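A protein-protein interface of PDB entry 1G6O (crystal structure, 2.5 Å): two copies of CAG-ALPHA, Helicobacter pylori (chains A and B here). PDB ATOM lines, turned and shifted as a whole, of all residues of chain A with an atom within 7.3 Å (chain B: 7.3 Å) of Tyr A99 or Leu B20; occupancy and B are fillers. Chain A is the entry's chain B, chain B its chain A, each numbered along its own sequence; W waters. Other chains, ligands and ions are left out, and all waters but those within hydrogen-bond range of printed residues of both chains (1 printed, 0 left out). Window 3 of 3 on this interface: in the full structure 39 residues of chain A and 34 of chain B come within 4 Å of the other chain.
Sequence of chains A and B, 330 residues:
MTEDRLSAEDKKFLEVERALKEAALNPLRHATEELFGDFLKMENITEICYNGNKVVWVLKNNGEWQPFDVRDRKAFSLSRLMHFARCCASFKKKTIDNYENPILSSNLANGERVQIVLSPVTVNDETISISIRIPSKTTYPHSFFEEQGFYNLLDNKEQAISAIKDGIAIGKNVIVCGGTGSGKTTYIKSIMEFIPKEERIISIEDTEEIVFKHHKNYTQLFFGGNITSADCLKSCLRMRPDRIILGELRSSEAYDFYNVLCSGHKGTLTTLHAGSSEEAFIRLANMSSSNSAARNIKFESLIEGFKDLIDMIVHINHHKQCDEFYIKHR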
ATOM      1  N   ILE A  96      40.831  22.665 -18.127  1.00  0.00           N
ATOM      2  CA  ILE A  96      39.864  21.665 -17.684  1.00  0.00           C
ATOM      3  C   ILE A  96      38.472  22.107 -18.184  1.00  0.00           C
ATOM      4  O   ILE A  96      38.067  23.254 -17.994  1.00  0.00           O
ATOM      5  CB  ILE A  96      39.886  21.495 -16.145  1.00  0.00           C
ATOM      6  CG1 ILE A  96      39.090  20.243 -15.760  1.00  0.00           C
ATOM      7  CG2 ILE A  96      39.327  22.719 -15.478  1.00  0.00           C
ATOM      8  CD1 ILE A  96      39.211  19.834 -14.317  1.00  0.00           C
ATOM      9  N   ASP A  97      37.753  21.195 -18.836  1.00  0.00           N
ATOM     10  CA  ASP A  97      36.436  21.488 -19.398  1.00  0.00           C
ATOM     11  C   ASP A  97      35.607  20.204 -19.536  1.00  0.00           C
ATOM     12  O   ASP A  97      36.108  19.102 -19.322  1.00  0.00           O
ATOM     13  CB  ASP A  97      36.628  22.136 -20.768  1.00  0.00           C
ATOM     14  CG  ASP A  97      37.445  21.259 -21.719  1.00  0.00           C
ATOM     15  OD1 ASP A  97      38.419  21.751 -22.360  1.00  0.00           O
ATOM     16  OD2 ASP A  97      37.121  20.054 -21.827  1.00  0.00           O
ATOM     17  N   ASN A  98      34.343  20.352 -19.924  1.00  0.00           N
ATOM     18  CA  ASN A  98      33.428  19.212 -20.081  1.00  0.00           C
ATOM     19  C   ASN A  98      33.441  18.569 -21.453  1.00  0.00           C
ATOM     20  O   ASN A  98      32.470  17.926 -21.843  1.00  0.00           O
ATOM     21  CB  ASN A  98      31.998  19.639 -19.795  1.00  0.00           C
ATOM     22  CG  ASN A  98      31.857  20.308 -18.455  1.00  0.00           C
ATOM     23  OD1 ASN A  98      31.718  21.531 -18.376  1.00  0.00           O
ATOM     24  ND2 ASN A  98      31.890  19.518 -17.390  1.00  0.00           N
ATOM     25  N   TYR A  99      34.539  18.747 -22.179  1.00  0.00           N
ATOM     26  CA  TYR A  99      34.664  18.206 -23.523  1.00  0.00           C
ATOM     27  C   TYR A  99      35.952  17.392 -23.677  1.00  0.00           C
ATOM     28  O   TYR A  99      35.983  16.192 -23.385  1.00  0.00           O
ATOM     29  CB  TYR A  99      34.603  19.346 -24.558  1.00  0.00           C
ATOM     30  CG  TYR A  99      33.252  20.047 -24.603  1.00  0.00           C
ATOM     31  CD1 TYR A  99      32.915  21.027 -23.669  1.00  0.00           C
ATOM     32  CD2 TYR A  99      32.278  19.661 -25.522  1.00  0.00           C
ATOM     33  CE1 TYR A  99      31.647  21.586 -23.643  1.00  0.00           C
ATOM     34  CE2 TYR A  99      31.012  20.218 -25.501  1.00  0.00           C
ATOM     35  CZ  TYR A  99      30.700  21.178 -24.557  1.00  0.00           C
ATOM     36  OH  TYR A  99      29.438  21.716 -24.519  1.00  0.00           O
ATOM     37  N   GLU A 100      37.021  18.029 -24.118  1.00  0.00           N
ATOM     38  CA  GLU A 100      38.259  17.307 -24.320  1.00  0.00           C
ATOM     39  C   GLU A 100      39.189  17.251 -23.112  1.00  0.00           C
ATOM     40  O   GLU A 100      40.236  16.632 -23.185  1.00  0.00           O
ATOM     41  CB  GLU A 100      39.016  17.915 -25.509  1.00  0.00           C
ATOM     42  CG  GLU A 100      38.360  17.678 -26.865  1.00  0.00           C
ATOM     43  CD  GLU A 100      38.482  16.229 -27.362  1.00  0.00           C
ATOM     44  OE1 GLU A 100      37.455  15.641 -27.795  1.00  0.00           O
ATOM     45  OE2 GLU A 100      39.605  15.656 -27.338  1.00  0.00           O
ATOM     46  N   ASN A 101      38.836  17.884 -22.003  1.00  0.00           N
ATOM     47  CA  ASN A 101      39.723  17.864 -20.841  1.00  0.00           C
ATOM     48  C   ASN A 101      38.951  17.725 -19.526  1.00  0.00           C
ATOM     49  O   ASN A 101      39.035  18.588 -18.660  1.00  0.00           O
ATOM     50  CB  ASN A 101      40.550  19.151 -20.807  1.00  0.00           C
ATOM     51  CG  ASN A 101      41.372  19.363 -22.077  1.00  0.00           C
ATOM     52  OD1 ASN A 101      42.298  18.614 -22.359  1.00  0.00           O
ATOM     53  ND2 ASN A 101      41.032  20.394 -22.843  1.00  0.00           N
ATOM     54  N   PRO A 102      38.176  16.641 -19.366  1.00  0.00           N
ATOM     55  CA  PRO A 102      37.387  16.403 -18.146  1.00  0.00           C
ATOM     56  C   PRO A 102      38.173  15.790 -16.975  1.00  0.00           C
ATOM     57  O   PRO A 102      37.705  15.767 -15.835  1.00  0.00           O
ATOM     58  CB  PRO A 102      36.271  15.490 -18.648  1.00  0.00           C
ATOM     59  CG  PRO A 102      36.990  14.654 -19.681  1.00  0.00           C
ATOM     60  CD  PRO A 102      37.815  15.677 -20.426  1.00  0.00           C
ATOM     61  N   ILE A 103      39.374  15.307 -17.287  1.00  0.00           N
ATOM     62  CA  ILE A 103      40.273  14.698 -16.313  1.00  0.00           C
ATOM     63  C   ILE A 103      41.517  15.571 -16.226  1.00  0.00           C
ATOM     64  O   ILE A 103      42.134  15.880 -17.246  1.00  0.00           O
ATOM     65  CB  ILE A 103      40.701  13.258 -16.740  1.00  0.00           C
ATOM     66  CG1 ILE A 103      39.479  12.333 -16.811  1.00  0.00           C
ATOM     67  CG2 ILE A 103      41.744  12.689 -15.762  1.00  0.00           C
ATOM     68  CD1 ILE A 103      39.830  10.904 -17.138  1.00  0.00           C
ATOM     69  N   LEU A 118      35.487  15.788 -14.237  1.00  0.00           N
ATOM     70  CA  LEU A 118      34.230  16.468 -14.498  1.00  0.00           C
ATOM     71  C   LEU A 118      33.346  15.635 -15.355  1.00  0.00           C
ATOM     72  O   LEU A 118      33.776  14.607 -15.871  1.00  0.00           O
ATOM     73  CB  LEU A 118      34.458  17.759 -15.261  1.00  0.00           C
ATOM     74  CG  LEU A 118      35.483  18.694 -14.656  1.00  0.00           C
ATOM     75  CD1 LEU A 118      35.592  19.824 -15.635  1.00  0.00           C
ATOM     76  CD2 LEU A 118      35.092  19.175 -13.250  1.00  0.00           C
ATOM     77  N   SER A 119      32.108  16.091 -15.505  1.00  0.00           N
ATOM     78  CA  SER A 119      31.149  15.434 -16.370  1.00  0.00           C
ATOM     79  C   SER A 119      31.776  15.674 -17.777  1.00  0.00           C
ATOM     80  O   SER A 119      32.461  16.687 -18.001  1.00  0.00           O
ATOM     81  CB  SER A 119      29.787  16.126 -16.195  1.00  0.00           C
ATOM     82  OG  SER A 119      28.804  15.658 -17.103  1.00  0.00           O
ATOM     83  N   PRO A 120      31.545  14.768 -18.751  1.00  0.00           N
ATOM     84  CA  PRO A 120      30.774  13.513 -18.787  1.00  0.00           C
ATOM     85  C   PRO A 120      31.386  12.269 -18.130  1.00  0.00           C
ATOM     86  O   PRO A 120      30.745  11.211 -18.050  1.00  0.00           O
ATOM     87  CB  PRO A 120      30.550  13.317 -20.284  1.00  0.00           C
ATOM     88  CG  PRO A 120      31.874  13.765 -20.855  1.00  0.00           C
ATOM     89  CD  PRO A 120      32.179  15.029 -20.062  1.00  0.00           C
ATOM     90  N   VAL A 121      32.618  12.404 -17.660  1.00  0.00           N
ATOM     91  CA  VAL A 121      33.298  11.295 -17.022  1.00  0.00           C
ATOM     92  C   VAL A 121      32.687  10.918 -15.662  1.00  0.00           C
ATOM     93  O   VAL A 121      32.533   9.726 -15.351  1.00  0.00           O
ATOM     94  CB  VAL A 121      34.781  11.596 -16.911  1.00  0.00           C
ATOM     95  CG1 VAL A 121      35.506  10.468 -16.192  1.00  0.00           C
ATOM     96  CG2 VAL A 121      35.337  11.723 -18.306  1.00  0.00           C
ATOM     97  N   LEU B  14      24.779  25.956 -14.625  1.00  0.00           N
ATOM     98  CA  LEU B  14      24.565  24.859 -15.576  1.00  0.00           C
ATOM     99  C   LEU B  14      23.711  25.226 -16.782  1.00  0.00           C
ATOM    100  O   LEU B  14      23.659  24.464 -17.748  1.00  0.00           O
ATOM    101  CB  LEU B  14      23.894  23.687 -14.864  1.00  0.00           C
ATOM    102  CG  LEU B  14      24.542  23.127 -13.603  1.00  0.00           C
ATOM    103  CD1 LEU B  14      23.515  22.342 -12.817  1.00  0.00           C
ATOM    104  CD2 LEU B  14      25.709  22.260 -13.982  1.00  0.00           C
ATOM    105  N   GLU B  15      23.045  26.382 -16.706  1.00  0.00           N
ATOM    106  CA  GLU B  15      22.155  26.894 -17.747  1.00  0.00           C
ATOM    107  C   GLU B  15      22.626  26.675 -19.190  1.00  0.00           C
ATOM    108  O   GLU B  15      21.904  26.073 -19.989  1.00  0.00           O
ATOM    109  CB  GLU B  15      21.893  28.388 -17.494  1.00  0.00           C
ATOM    110  CG  GLU B  15      20.753  28.988 -18.338  1.00  0.00           C
ATOM    111  CD  GLU B  15      20.516  30.511 -18.142  1.00  0.00           C
ATOM    112  OE1 GLU B  15      21.227  31.180 -17.340  1.00  0.00           O
ATOM    113  OE2 GLU B  15      19.593  31.033 -18.815  1.00  0.00           O
ATOM    114  N   VAL B  16      23.823  27.157 -19.521  1.00  0.00           N
ATOM    115  CA  VAL B  16      24.383  27.035 -20.874  1.00  0.00           C
ATOM    116  C   VAL B  16      24.696  25.637 -21.370  1.00  0.00           C
ATOM    117  O   VAL B  16      24.450  25.300 -22.539  1.00  0.00           O
ATOM    118  CB  VAL B  16      25.685  27.811 -21.009  1.00  0.00           C
ATOM    119  CG1 VAL B  16      26.392  27.416 -22.322  1.00  0.00           C
ATOM    120  CG2 VAL B  16      25.391  29.295 -20.941  1.00  0.00           C
ATOM    121  N   GLU B  17      25.293  24.836 -20.500  1.00  0.00           N
ATOM    122  CA  GLU B  17      25.639  23.466 -20.855  1.00  0.00           C
ATOM    123  C   GLU B  17      24.357  22.598 -20.936  1.00  0.00           C
ATOM    124  O   GLU B  17      24.222  21.764 -21.824  1.00  0.00           O
ATOM    125  CB  GLU B  17      26.655  22.921 -19.831  1.00  0.00           C
ATOM    126  CG  GLU B  17      27.429  21.667 -20.244  1.00  0.00           C
ATOM    127  CD  GLU B  17      28.252  21.830 -21.524  1.00  0.00           C
ATOM    128  OE1 GLU B  17      28.457  22.976 -21.967  1.00  0.00           O
ATOM    129  OE2 GLU B  17      28.705  20.798 -22.081  1.00  0.00           O
ATOM    130  N   ARG B  18      23.402  22.815 -20.039  1.00  0.00           N
ATOM    131  CA  ARG B  18      22.174  22.025 -20.081  1.00  0.00           C
ATOM    132  C   ARG B  18      21.392  22.249 -21.359  1.00  0.00           C
ATOM    133  O   ARG B  18      20.931  21.294 -21.999  1.00  0.00           O
ATOM    134  CB  ARG B  18      21.290  22.321 -18.863  1.00  0.00           C
ATOM    135  CG  ARG B  18      21.817  21.634 -17.622  1.00  0.00           C
ATOM    136  CD  ARG B  18      20.920  21.723 -16.411  1.00  0.00           C
ATOM    137  NE  ARG B  18      21.251  20.643 -15.488  1.00  0.00           N
ATOM    138  CZ  ARG B  18      20.663  20.449 -14.316  1.00  0.00           C
ATOM    139  NH1 ARG B  18      19.707  21.281 -13.927  1.00  0.00           N
ATOM    140  NH2 ARG B  18      21.015  19.416 -13.546  1.00  0.00           N
ATOM    141  N   ALA B  19      21.264  23.532 -21.708  1.00  0.00           N
ATOM    142  CA  ALA B  19      20.563  24.019 -22.894  1.00  0.00           C
ATOM    143  C   ALA B  19      21.129  23.369 -24.130  1.00  0.00           C
ATOM    144  O   ALA B  19      20.386  22.950 -25.007  1.00  0.00           O
ATOM    145  CB  ALA B  19      20.719  25.521 -22.987  1.00  0.00           C
ATOM    146  N   LEU B  20      22.451  23.297 -24.201  1.00  0.00           N
ATOM    147  CA  LEU B  20      23.120  22.683 -25.335  1.00  0.00           C
ATOM    148  C   LEU B  20      22.837  21.198 -25.425  1.00  0.00           C
ATOM    149  O   LEU B  20      22.719  20.670 -26.524  1.00  0.00           O
ATOM    150  CB  LEU B  20      24.631  22.896 -25.260  1.00  0.00           C
ATOM    151  CG  LEU B  20      25.097  24.343 -25.440  1.00  0.00           C
ATOM    152  CD1 LEU B  20      26.597  24.428 -25.225  1.00  0.00           C
ATOM    153  CD2 LEU B  20      24.739  24.832 -26.845  1.00  0.00           C
ATOM    154  N   LYS B  21      22.744  20.507 -24.289  1.00  0.00           N
ATOM    155  CA  LYS B  21      22.454  19.065 -24.329  1.00  0.00           C
ATOM    156  C   LYS B  21      20.991  18.869 -24.746  1.00  0.00           C
ATOM    157  O   LYS B  21      20.691  18.054 -25.618  1.00  0.00           O
ATOM    158  CB  LYS B  21      22.670  18.378 -22.954  1.00  0.00           C
ATOM    159  CG  LYS B  21      24.045  18.534 -22.300  1.00  0.00           C
ATOM    160  CD  LYS B  21      25.171  18.178 -23.235  1.00  0.00           C
ATOM    161  CE  LYS B  21      26.522  18.486 -22.629  1.00  0.00           C
ATOM    162  NZ  LYS B  21      27.594  18.299 -23.651  1.00  0.00           N
ATOM    163  N   GLU B  22      20.086  19.625 -24.135  1.00  0.00           N
ATOM    164  CA  GLU B  22      18.686  19.485 -24.470  1.00  0.00           C
ATOM    165  C   GLU B  22      18.390  19.737 -25.963  1.00  0.00           C
ATOM    166  O   GLU B  22      17.560  19.063 -26.564  1.00  0.00           O
ATOM    167  CB  GLU B  22      17.847  20.392 -23.580  1.00  0.00           C
ATOM    168  CG  GLU B  22      16.388  20.084 -23.668  1.00  0.00           C
ATOM    169  CD  GLU B  22      15.545  20.970 -22.783  1.00  0.00           C
ATOM    170  OE1 GLU B  22      16.125  21.615 -21.878  1.00  0.00           O
ATOM    171  OE2 GLU B  22      14.305  21.013 -22.974  1.00  0.00           O
ATOM    172  N   ALA B  23      19.075  20.684 -26.583  1.00  0.00           N
ATOM    173  CA  ALA B  23      18.842  20.944 -28.005  1.00  0.00           C
ATOM    174  C   ALA B  23      19.275  19.749 -28.867  1.00  0.00           C
ATOM    175  O   ALA B  23      18.662  19.430 -29.892  1.00  0.00           O
ATOM    176  CB  ALA B  23      19.595  22.164 -28.422  1.00  0.00           C
ATOM    177  N   ALA B  24      20.340  19.090 -28.426  1.00  0.00           N
ATOM    178  CA  ALA B  24      20.905  17.941 -29.116  1.00  0.00           C
ATOM    179  C   ALA B  24      20.207  16.626 -28.771  1.00  0.00           C
ATOM    180  O   ALA B  24      20.081  15.726 -29.607  1.00  0.00           O
ATOM    181  CB  ALA B  24      22.387  17.834 -28.782  1.00  0.00           C
ATOM    182  N   LEU B  25      19.731  16.509 -27.545  1.00  0.00           N
ATOM    183  CA  LEU B  25      19.114  15.266 -27.134  1.00  0.00           C
ATOM    184  C   LEU B  25      17.597  15.144 -27.351  1.00  0.00           C
ATOM    185  O   LEU B  25      17.084  14.040 -27.540  1.00  0.00           O
ATOM    186  CB  LEU B  25      19.474  15.012 -25.667  1.00  0.00           C
ATOM    187  CG  LEU B  25      19.243  13.609 -25.098  1.00  0.00           C
ATOM    188  CD1 LEU B  25      20.063  12.556 -25.865  1.00  0.00           C
ATOM    189  CD2 LEU B  25      19.624  13.624 -23.623  1.00  0.00           C
ATOM    190  N   LYS B  93      28.034  13.128 -32.052  1.00  0.00           N
ATOM    191  CA  LYS B  93      28.803  13.901 -33.013  1.00  0.00           C
ATOM    192  C   LYS B  93      29.379  13.037 -34.136  1.00  0.00           C
ATOM    193  O   LYS B  93      30.569  13.127 -34.467  1.00  0.00           O
ATOM    194  CB  LYS B  93      29.933  14.666 -32.302  1.00  0.00           C
ATOM    195  CG  LYS B  93      29.462  15.633 -31.208  1.00  0.00           C
ATOM    196  CD  LYS B  93      30.660  16.332 -30.552  1.00  0.00           C
ATOM    197  CE  LYS B  93      30.223  17.344 -29.462  1.00  0.00           C
ATOM    198  NZ  LYS B  93      30.529  16.969 -28.027  1.00  0.00           N
ATOM    199  N   ASN B 226      36.229  10.313 -26.849  1.00  0.00           N
ATOM    200  CA  ASN B 226      37.677  10.504 -26.762  1.00  0.00           C
ATOM    201  C   ASN B 226      38.334  10.010 -25.463  1.00  0.00           C
ATOM    202  O   ASN B 226      39.561   9.921 -25.405  1.00  0.00           O
ATOM    203  CB  ASN B 226      38.024  11.994 -26.964  1.00  0.00           C
ATOM    204  CG  ASN B 226      37.714  12.488 -28.374  1.00  0.00           C
ATOM    205  OD1 ASN B 226      38.464  12.220 -29.319  1.00  0.00           O
ATOM    206  ND2 ASN B 226      36.597  13.199 -28.524  1.00  0.00           N
ATOM    207  N   ILE B 227      37.535   9.711 -24.432  1.00  0.00           N
ATOM    208  CA  ILE B 227      38.044   9.224 -23.129  1.00  0.00           C
ATOM    209  C   ILE B 227      37.972   7.707 -23.124  1.00  0.00           C
ATOM    210  O   ILE B 227      36.891   7.119 -23.100  1.00  0.00           O
ATOM    211  CB  ILE B 227      37.201   9.746 -21.934  1.00  0.00           C
ATOM    212  CG1 ILE B 227      37.162  11.280 -21.937  1.00  0.00           C
ATOM    213  CG2 ILE B 227      37.801   9.267 -20.634  1.00  0.00           C
ATOM    214  CD1 ILE B 227      38.529  11.938 -21.737  1.00  0.00           C
HETATM  215  O   HOH W   1      30.025  17.546 -22.496  1.00  0.00           O
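Hydrophobic or aromatic side chains of chain A within 4 Å of the printed part of chain B: Tyr A99 and Pro A102.
Of the 15 printed residues of chain B, 5 touch a printed residue of chain A.
Hydrophobic or aromatic side chains of chain B that line the printed part of chain A: Leu B20 and Ile B227.
Tyr A99 touches Leu B20.
Tyr A99 touches Lys B21 (OH to NZ, 3.98 Å).
Pro A102 touches Ile B227.
No position is printed for both chains.
The side-chain amino group (NZ) of Lys B21 lies within salt-bridge range of the side-chain carboxylate (OE2) of Glu B17.
The backbone NH of Tyr A99 lies within hydrogen-bond range of the side-chain carboxylate of Asp A97, at 2.9 Å.
OD2 of Asp A97 lies within hydrogen-bond range of N of Glu A100 (3.1 Å).
N of Leu A118 lies within hydrogen-bond range of O of Pro A102 (2.7 Å).
Of the printed residues of chain B, Tyr A99 touches Glu B17 (2.7 Å), Leu B20 (3.99 Å) and Lys B21 (3.98 Å).
Of the printed residues of chain A, Leu B20 touches Tyr A99 (3.99 Å).
No residue of chain A comes within 4 Å of Ala B19.
Printed residues of chain A within 4 Å of Ile B227: Pro A102 (3.7 Å).
Printed residues of chain A within 4 Å of Lys B21: Tyr A99.
Ile A96 touches none of the printed residues of chain B.
Leu B14 touches none of the printed residues of chain A.
The nearest printed residue of chain B that does not touch Tyr A99 is Lys B93 (4.1 Å).
Water W1 bridges the backbone carbonyl oxygen of Asn A98 and the side-chain amino group of Lys B21.
The side-chain carboxylate of Glu B17 sits at hydrogen-bond distance from the side-chain hydroxyl of Tyr A99, 2.7 Å away.
The side-chain amide nitrogen (ND2) of Asn B226 lies within hydrogen-bond range of the side-chain carboxylate (OE1) of Glu A100, at 2.7 Å.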
